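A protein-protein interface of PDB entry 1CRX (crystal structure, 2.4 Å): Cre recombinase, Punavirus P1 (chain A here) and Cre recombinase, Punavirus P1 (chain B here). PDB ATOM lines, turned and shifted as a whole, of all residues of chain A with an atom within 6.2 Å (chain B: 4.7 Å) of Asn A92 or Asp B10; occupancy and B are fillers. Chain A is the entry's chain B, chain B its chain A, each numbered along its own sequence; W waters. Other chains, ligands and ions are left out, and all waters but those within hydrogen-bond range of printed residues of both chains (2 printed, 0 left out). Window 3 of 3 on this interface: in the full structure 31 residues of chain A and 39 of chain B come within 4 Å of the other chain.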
ATOM      1  N   GLU A  50       0.149  -3.149 -20.455  1.00  0.00           N
ATOM      2  CA  GLU A  50      -0.991  -2.446 -19.893  1.00  0.00           C
ATOM      3  C   GLU A  50      -1.958  -2.076 -21.003  1.00  0.00           C
ATOM      4  O   GLU A  50      -3.180  -2.073 -20.814  1.00  0.00           O
ATOM      5  CB  GLU A  50      -0.521  -1.193 -19.142  1.00  0.00           C
ATOM      6  CG  GLU A  50       0.048  -1.478 -17.754  1.00  0.00           C
ATOM      7  CD  GLU A  50      -0.984  -2.083 -16.813  1.00  0.00           C
ATOM      8  OE1 GLU A  50      -2.154  -1.643 -16.848  1.00  0.00           O
ATOM      9  OE2 GLU A  50      -0.620  -3.000 -16.045  1.00  0.00           O
ATOM     10  N   ARG A  53      -3.687  -5.198 -22.214  1.00  0.00           N
ATOM     11  CA  ARG A  53      -4.696  -5.578 -21.232  1.00  0.00           C
ATOM     12  C   ARG A  53      -6.006  -4.837 -21.485  1.00  0.00           C
ATOM     13  O   ARG A  53      -7.073  -5.443 -21.486  1.00  0.00           O
ATOM     14  CB  ARG A  53      -4.208  -5.274 -19.819  1.00  0.00           C
ATOM     15  CG  ARG A  53      -4.707  -6.254 -18.812  1.00  0.00           C
ATOM     16  CD  ARG A  53      -4.593  -5.701 -17.426  1.00  0.00           C
ATOM     17  NE  ARG A  53      -5.537  -4.619 -17.239  1.00  0.00           N
ATOM     18  CZ  ARG A  53      -6.503  -4.626 -16.333  1.00  0.00           C
ATOM     19  NH1 ARG A  53      -6.653  -5.665 -15.528  1.00  0.00           N
ATOM     20  NH2 ARG A  53      -7.318  -3.589 -16.238  1.00  0.00           N
ATOM     21  N   PRO A  88       3.522 -10.030 -24.890  1.00  0.00           N
ATOM     22  CA  PRO A  88       2.621  -9.401 -23.924  1.00  0.00           C
ATOM     23  C   PRO A  88       2.230 -10.363 -22.787  1.00  0.00           C
ATOM     24  O   PRO A  88       2.130  -9.961 -21.628  1.00  0.00           O
ATOM     25  CB  PRO A  88       1.429  -8.981 -24.784  1.00  0.00           C
ATOM     26  CG  PRO A  88       2.023  -8.774 -26.136  1.00  0.00           C
ATOM     27  CD  PRO A  88       3.041  -9.866 -26.271  1.00  0.00           C
ATOM     28  N   SER A  89       2.028 -11.637 -23.125  1.00  0.00           N
ATOM     29  CA  SER A  89       1.652 -12.650 -22.146  1.00  0.00           C
ATOM     30  C   SER A  89       2.753 -12.865 -21.125  1.00  0.00           C
ATOM     31  O   SER A  89       2.561 -13.564 -20.131  1.00  0.00           O
ATOM     32  CB  SER A  89       1.359 -13.977 -22.842  1.00  0.00           C
ATOM     33  OG  SER A  89      -0.033 -14.184 -22.960  1.00  0.00           O
ATOM     34  N   ASP A  90       3.912 -12.267 -21.374  1.00  0.00           N
ATOM     35  CA  ASP A  90       5.044 -12.402 -20.466  1.00  0.00           C
ATOM     36  C   ASP A  90       4.817 -11.554 -19.209  1.00  0.00           C
ATOM     37  O   ASP A  90       5.418 -11.791 -18.163  1.00  0.00           O
ATOM     38  CB  ASP A  90       6.334 -11.972 -21.176  1.00  0.00           C
ATOM     39  CG  ASP A  90       6.903 -13.063 -22.077  1.00  0.00           C
ATOM     40  OD1 ASP A  90       6.740 -14.257 -21.749  1.00  0.00           O
ATOM     41  OD2 ASP A  90       7.517 -12.730 -23.116  1.00  0.00           O
ATOM     42  N   SER A  91       3.924 -10.577 -19.324  1.00  0.00           N
ATOM     43  CA  SER A  91       3.608  -9.682 -18.225  1.00  0.00           C
ATOM     44  C   SER A  91       2.431 -10.149 -17.379  1.00  0.00           C
ATOM     45  O   SER A  91       1.477 -10.722 -17.888  1.00  0.00           O
ATOM     46  CB  SER A  91       3.307  -8.295 -18.778  1.00  0.00           C
ATOM     47  OG  SER A  91       1.983  -8.245 -19.275  1.00  0.00           O
ATOM     48  N   ASN A  92       2.507  -9.876 -16.081  1.00  0.00           N
ATOM     49  CA  ASN A  92       1.467 -10.233 -15.117  1.00  0.00           C
ATOM     50  C   ASN A  92       0.109  -9.685 -15.544  1.00  0.00           C
ATOM     51  O   ASN A  92      -0.905 -10.389 -15.526  1.00  0.00           O
ATOM     52  CB  ASN A  92       1.808  -9.623 -13.759  1.00  0.00           C
ATOM     53  CG  ASN A  92       2.179 -10.655 -12.725  1.00  0.00           C
ATOM     54  OD1 ASN A  92       2.672 -11.735 -13.055  1.00  0.00           O
ATOM     55  ND2 ASN A  92       1.945 -10.324 -11.452  1.00  0.00           N
ATOM     56  N   ALA A  93       0.097  -8.410 -15.903  1.00  0.00           N
ATOM     57  CA  ALA A  93      -1.127  -7.748 -16.302  1.00  0.00           C
ATOM     58  C   ALA A  93      -1.876  -8.504 -17.381  1.00  0.00           C
ATOM     59  O   ALA A  93      -3.078  -8.747 -17.257  1.00  0.00           O
ATOM     60  CB  ALA A  93      -0.817  -6.338 -16.780  1.00  0.00           C
ATOM     61  N   VAL A  94      -1.165  -8.880 -18.439  1.00  0.00           N
ATOM     62  CA  VAL A  94      -1.802  -9.560 -19.557  1.00  0.00           C
ATOM     63  C   VAL A  94      -2.209 -10.985 -19.264  1.00  0.00           C
ATOM     64  O   VAL A  94      -3.290 -11.405 -19.662  1.00  0.00           O
ATOM     65  CB  VAL A  94      -0.917  -9.511 -20.821  1.00  0.00           C
ATOM     66  CG1 VAL A  94      -1.620 -10.176 -21.976  1.00  0.00           C
ATOM     67  CG2 VAL A  94      -0.650  -8.075 -21.185  1.00  0.00           C
ATOM     68  N   SER A  95      -1.363 -11.726 -18.557  1.00  0.00           N
ATOM     69  CA  SER A  95      -1.681 -13.112 -18.225  1.00  0.00           C
ATOM     70  C   SER A  95      -2.864 -13.185 -17.265  1.00  0.00           C
ATOM     71  O   SER A  95      -3.757 -14.015 -17.431  1.00  0.00           O
ATOM     72  CB  SER A  95      -0.471 -13.807 -17.600  1.00  0.00           C
ATOM     73  OG  SER A  95       0.127 -12.983 -16.622  1.00  0.00           O
ATOM     74  N   LEU A  96      -2.888 -12.304 -16.273  1.00  0.00           N
ATOM     75  CA  LEU A  96      -3.977 -12.312 -15.310  1.00  0.00           C
ATOM     76  C   LEU A  96      -5.310 -11.948 -15.943  1.00  0.00           C
ATOM     77  O   LEU A  96      -6.308 -12.623 -15.728  1.00  0.00           O
ATOM     78  CB  LEU A  96      -3.670 -11.353 -14.154  1.00  0.00           C
ATOM     79  CG  LEU A  96      -2.515 -11.780 -13.237  1.00  0.00           C
ATOM     80  CD1 LEU A  96      -2.097 -10.643 -12.311  1.00  0.00           C
ATOM     81  CD2 LEU A  96      -2.950 -12.987 -12.427  1.00  0.00           C
ATOM     82  N   VAL A  97      -5.339 -10.887 -16.731  1.00  0.00           N
ATOM     83  CA  VAL A  97      -6.598 -10.470 -17.341  1.00  0.00           C
ATOM     84  C   VAL A  97      -7.184 -11.474 -18.303  1.00  0.00           C
ATOM     85  O   VAL A  97      -8.397 -11.533 -18.462  1.00  0.00           O
ATOM     86  CB  VAL A  97      -6.463  -9.142 -18.085  1.00  0.00           C
ATOM     87  CG1 VAL A  97      -5.797  -9.359 -19.434  1.00  0.00           C
ATOM     88  CG2 VAL A  97      -7.827  -8.526 -18.248  1.00  0.00           C
ATOM     89  N   LYS B   6       4.306  -3.304  -7.925  1.00  0.00           N
ATOM     90  CA  LYS B   6       3.447  -3.252  -9.099  1.00  0.00           C
ATOM     91  C   LYS B   6       2.777  -4.591  -9.378  1.00  0.00           C
ATOM     92  O   LYS B   6       1.590  -4.647  -9.700  1.00  0.00           O
ATOM     93  CB  LYS B   6       4.265  -2.815 -10.318  1.00  0.00           C
ATOM     94  CG  LYS B   6       3.818  -3.432 -11.633  1.00  0.00           C
ATOM     95  CD  LYS B   6       2.744  -2.599 -12.310  1.00  0.00           C
ATOM     96  CE  LYS B   6       2.680  -2.900 -13.794  1.00  0.00           C
ATOM     97  NZ  LYS B   6       1.376  -3.509 -14.166  1.00  0.00           N
ATOM     98  N   ASN B   7       3.536  -5.671  -9.251  1.00  0.00           N
ATOM     99  CA  ASN B   7       3.008  -7.003  -9.512  1.00  0.00           C
ATOM    100  C   ASN B   7       1.928  -7.413  -8.514  1.00  0.00           C
ATOM    101  O   ASN B   7       1.032  -8.190  -8.837  1.00  0.00           O
ATOM    102  CB  ASN B   7       4.159  -8.010  -9.533  1.00  0.00           C
ATOM    103  CG  ASN B   7       4.975  -7.926 -10.820  1.00  0.00           C
ATOM    104  OD1 ASN B   7       4.410  -7.799 -11.911  1.00  0.00           O
ATOM    105  ND2 ASN B   7       6.300  -7.987 -10.702  1.00  0.00           N
ATOM    106  N   LEU B   8       2.013  -6.882  -7.304  1.00  0.00           N
ATOM    107  CA  LEU B   8       1.018  -7.173  -6.286  1.00  0.00           C
ATOM    108  C   LEU B   8      -0.243  -6.440  -6.707  1.00  0.00           C
ATOM    109  O   LEU B   8      -1.358  -6.936  -6.529  1.00  0.00           O
ATOM    110  CB  LEU B   8       1.474  -6.635  -4.927  1.00  0.00           C
ATOM    111  CG  LEU B   8       2.294  -7.480  -3.949  1.00  0.00           C
ATOM    112  CD1 LEU B   8       2.668  -8.825  -4.559  1.00  0.00           C
ATOM    113  CD2 LEU B   8       3.542  -6.702  -3.563  1.00  0.00           C
ATOM    114  N   MET B   9      -0.047  -5.242  -7.259  1.00  0.00           N
ATOM    115  CA  MET B   9      -1.140  -4.388  -7.720  1.00  0.00           C
ATOM    116  C   MET B   9      -1.889  -5.060  -8.872  1.00  0.00           C
ATOM    117  O   MET B   9      -3.116  -4.964  -8.969  1.00  0.00           O
ATOM    118  CB  MET B   9      -0.587  -3.021  -8.154  1.00  0.00           C
ATOM    119  CG  MET B   9      -0.792  -1.910  -7.107  1.00  0.00           C
ATOM    120  SD  MET B   9       0.343  -0.464  -7.186  1.00  0.00           S
ATOM    121  CE  MET B   9      -0.647   0.755  -6.362  1.00  0.00           C
ATOM    122  N   ASP B  10      -1.139  -5.743  -9.736  1.00  0.00           N
ATOM    123  CA  ASP B  10      -1.712  -6.468 -10.868  1.00  0.00           C
ATOM    124  C   ASP B  10      -2.738  -7.462 -10.333  1.00  0.00           C
ATOM    125  O   ASP B  10      -3.911  -7.437 -10.705  1.00  0.00           O
ATOM    126  CB  ASP B  10      -0.617  -7.246 -11.608  1.00  0.00           C
ATOM    127  CG  ASP B  10       0.235  -6.362 -12.488  1.00  0.00           C
ATOM    128  OD1 ASP B  10      -0.177  -5.227 -12.789  1.00  0.00           O
ATOM    129  OD2 ASP B  10       1.329  -6.801 -12.888  1.00  0.00           O
ATOM    130  N   MET B  11      -2.263  -8.330  -9.445  1.00  0.00           N
ATOM    131  CA  MET B  11      -3.068  -9.370  -8.818  1.00  0.00           C
ATOM    132  C   MET B  11      -4.397  -8.916  -8.204  1.00  0.00           C
ATOM    133  O   MET B  11      -5.460  -9.460  -8.520  1.00  0.00           O
ATOM    134  CB  MET B  11      -2.235 -10.067  -7.749  1.00  0.00           C
ATOM    135  CG  MET B  11      -1.938 -11.516  -8.048  1.00  0.00           C
ATOM    136  SD  MET B  11      -0.921 -12.224  -6.758  1.00  0.00           S
ATOM    137  CE  MET B  11       0.527 -11.185  -6.903  1.00  0.00           C
ATOM    138  N   PHE B  12      -4.354  -7.937  -7.312  1.00  0.00           N
ATOM    139  CA  PHE B  12      -5.595  -7.480  -6.716  1.00  0.00           C
ATOM    140  C   PHE B  12      -6.490  -6.866  -7.783  1.00  0.00           C
ATOM    141  O   PHE B  12      -7.709  -6.909  -7.675  1.00  0.00           O
ATOM    142  CB  PHE B  12      -5.315  -6.465  -5.607  1.00  0.00           C
ATOM    143  CG  PHE B  12      -6.519  -6.144  -4.745  1.00  0.00           C
ATOM    144  CD1 PHE B  12      -7.631  -5.492  -5.281  1.00  0.00           C
ATOM    145  CD2 PHE B  12      -6.520  -6.453  -3.388  1.00  0.00           C
ATOM    146  CE1 PHE B  12      -8.723  -5.149  -4.480  1.00  0.00           C
ATOM    147  CE2 PHE B  12      -7.609  -6.112  -2.578  1.00  0.00           C
ATOM    148  CZ  PHE B  12      -8.711  -5.457  -3.131  1.00  0.00           C
ATOM    149  N   ARG B  13      -5.900  -6.297  -8.828  1.00  0.00           N
ATOM    150  CA  ARG B  13      -6.724  -5.701  -9.875  1.00  0.00           C
ATOM    151  C   ARG B  13      -7.507  -6.789 -10.604  1.00  0.00           C
ATOM    152  O   ARG B  13      -8.711  -6.666 -10.831  1.00  0.00           O
ATOM    153  CB  ARG B  13      -5.865  -4.939 -10.878  1.00  0.00           C
ATOM    154  CG  ARG B  13      -6.695  -4.170 -11.901  1.00  0.00           C
ATOM    155  CD  ARG B  13      -5.819  -3.437 -12.895  1.00  0.00           C
ATOM    156  NE  ARG B  13      -4.636  -4.213 -13.259  1.00  0.00           N
ATOM    157  CZ  ARG B  13      -3.777  -3.809 -14.178  1.00  0.00           C
ATOM    158  NH1 ARG B  13      -3.994  -2.654 -14.794  1.00  0.00           N
ATOM    159  NH2 ARG B  13      -2.729  -4.555 -14.503  1.00  0.00           N
ATOM    160  N   ASP B  14      -6.812  -7.861 -10.967  1.00  0.00           N
ATOM    161  CA  ASP B  14      -7.444  -8.980 -11.660  1.00  0.00           C
ATOM    162  C   ASP B  14      -7.525 -10.140 -10.681  1.00  0.00           C
ATOM    163  O   ASP B  14      -7.166 -11.269 -11.007  1.00  0.00           O
ATOM    164  CB  ASP B  14      -6.631  -9.396 -12.894  1.00  0.00           C
ATOM    165  CG  ASP B  14      -6.611  -8.326 -13.976  1.00  0.00           C
ATOM    166  OD1 ASP B  14      -7.662  -7.708 -14.230  1.00  0.00           O
ATOM    167  OD2 ASP B  14      -5.541  -8.105 -14.581  1.00  0.00           O
ATOM    168  N   ARG B  82       5.090 -14.816  -9.804  1.00  0.00           N
ATOM    169  CA  ARG B  82       4.270 -13.708 -10.255  1.00  0.00           C
ATOM    170  C   ARG B  82       5.046 -12.410 -10.048  1.00  0.00           C
ATOM    171  O   ARG B  82       5.291 -11.677 -11.004  1.00  0.00           O
ATOM    172  CB  ARG B  82       2.952 -13.695  -9.491  1.00  0.00           C
ATOM    173  CG  ARG B  82       2.011 -14.806  -9.924  1.00  0.00           C
ATOM    174  CD  ARG B  82       0.796 -14.244 -10.619  1.00  0.00           C
ATOM    175  NE  ARG B  82       0.117 -15.231 -11.454  1.00  0.00           N
ATOM    176  CZ  ARG B  82       0.068 -15.176 -12.782  1.00  0.00           C
ATOM    177  NH1 ARG B  82       0.661 -14.183 -13.432  1.00  0.00           N
ATOM    178  NH2 ARG B  82      -0.591 -16.102 -13.465  1.00  0.00           N
HETATM  179  O   HOH W   1      -4.581  -2.073 -17.817  1.00  0.00           O
HETATM  180  O   HOH W   2       2.799 -10.524  -8.549  1.00  0.00           O
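The guanidinium group (NH1) of Arg A53 is in salt-bridge range of the side-chain carboxylate (OD1) of Asp B14 (2.6 Å).
The guanidinium group (NH1) of Arg B82 lies within hydrogen-bond range of the side-chain hydroxyl (OG) of Ser A95 (3.4 Å).
The guanidinium group (NH1) of Arg B82 sits at hydrogen-bond distance from the side-chain amide oxygen (OD1) of Asn A92 (3.2 Å).
NH1 of Arg A53 lies close to NE of Arg B13.
The side-chain amino group (NZ) of Lys B6 is in salt-bridge range of the side-chain carboxylate (OE2) of Glu A50 (2.8 Å).
OE1 of Glu A50 lies within salt-bridge range of NH1 of Arg B13 (2.9 Å).
The backbone carbonyl oxygen (O) of Asn B7 sits at hydrogen-bond distance from the side-chain amide nitrogen (ND2) of Asn A92, 3.5 Å away.
The backbone carbonyl oxygen (O) of Ser A91 lies within hydrogen-bond range of the side-chain hydroxyl (OG) of Ser A95 (2.9 Å).
O of Asn A92 sits at hydrogen-bond distance from OG of Ser A95 (3.0 Å).
OD1 of Asp B10 lies within salt-bridge range of NH2 of Arg B13.
The side-chain amide oxygen (OD1) of Asn B7 sits close to the side-chain carboxylate (OD2) of Asp B10, 3.4 Å away.
NZ of Lys B6 lies within salt-bridge range of OD1 of Asp B10 (2.7 Å).
Asp B10 touches Glu A50 (OD1 to OE2, 3.97 Å).
Asn A92 touches Asp B10.
Ala A93 touches Asp B10.
Arg B13 touches Ala A93.
Ala A93 touches Asp B14 (O to OD2, 3.7 Å).
Leu A96 touches Asp B10 (CD1 to CB, 3.8 Å).
Met B11 touches Leu A96 (N to CD1, 3.7 Å).
Leu A96 touches Asp B14.
CD2 of Leu A96 touches CZ of Arg B82 (3.7 Å).
N of Val A97 touches OD2 of Asp B14, at 3.5 Å.
Asn A92 touches three residues of chain B.
Of the printed residues of chain A, Asp B10 touches Glu A50 (3.97 Å), Asn A92 (3.0 Å), Ala A93 (3.6 Å) and Leu A96 (3.8 Å).
Printed residues of chain B within 4 Å of Ser A95: Arg B82 (3.4 Å).
Of the printed residues of chain A, Asn B7 touches Asn A92.
Of the printed residues of chain A, Arg B13 touches Glu A50, Arg A53 and Ala A93.
Of the printed residues of chain A, Asp B14 touches Arg A53 (2.6 Å), Ala A93 (3.7 Å), Leu A96 (3.8 Å) and Val A97 (3.5 Å).
The nearest printed residue of chain B that does not touch Asn A92 is Met B11 (4.8 Å).
The nearest residue of chain A that does not touch Asp B10 is Ser A91 (5.7 Å).
The nearest printed residue of chain A that does not touch Arg B13 is Asn A92 (6.0 Å).
Printed residues of chain A that touch a printed residue of chain B: Glu A50, Arg A53, Asn A92, Ala A93, Ser A95, Leu A96 and Val A97.
Hydrophobic or aromatic side chains of chain A within 4 Å of the printed part of chain B: Ala A93, Leu A96 and Val A97.
Along chain A the printed residues that touch a printed residue of chain B span positions 50 to 97.
Of the 10 printed residues of chain B, 7 touch a printed residue of chain A.
Along chain B the printed residues that touch a printed residue of chain A span positions 6 to 82.
Among the printed residues, 17 pairs touch across the chains.
Water W1 lies within hydrogen-bond range of OE1 of Glu A50, NE of Arg A53 and NH1 of Arg B13.
Water W2 bridges O of Asn B7 and ND2 of Asn A92.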
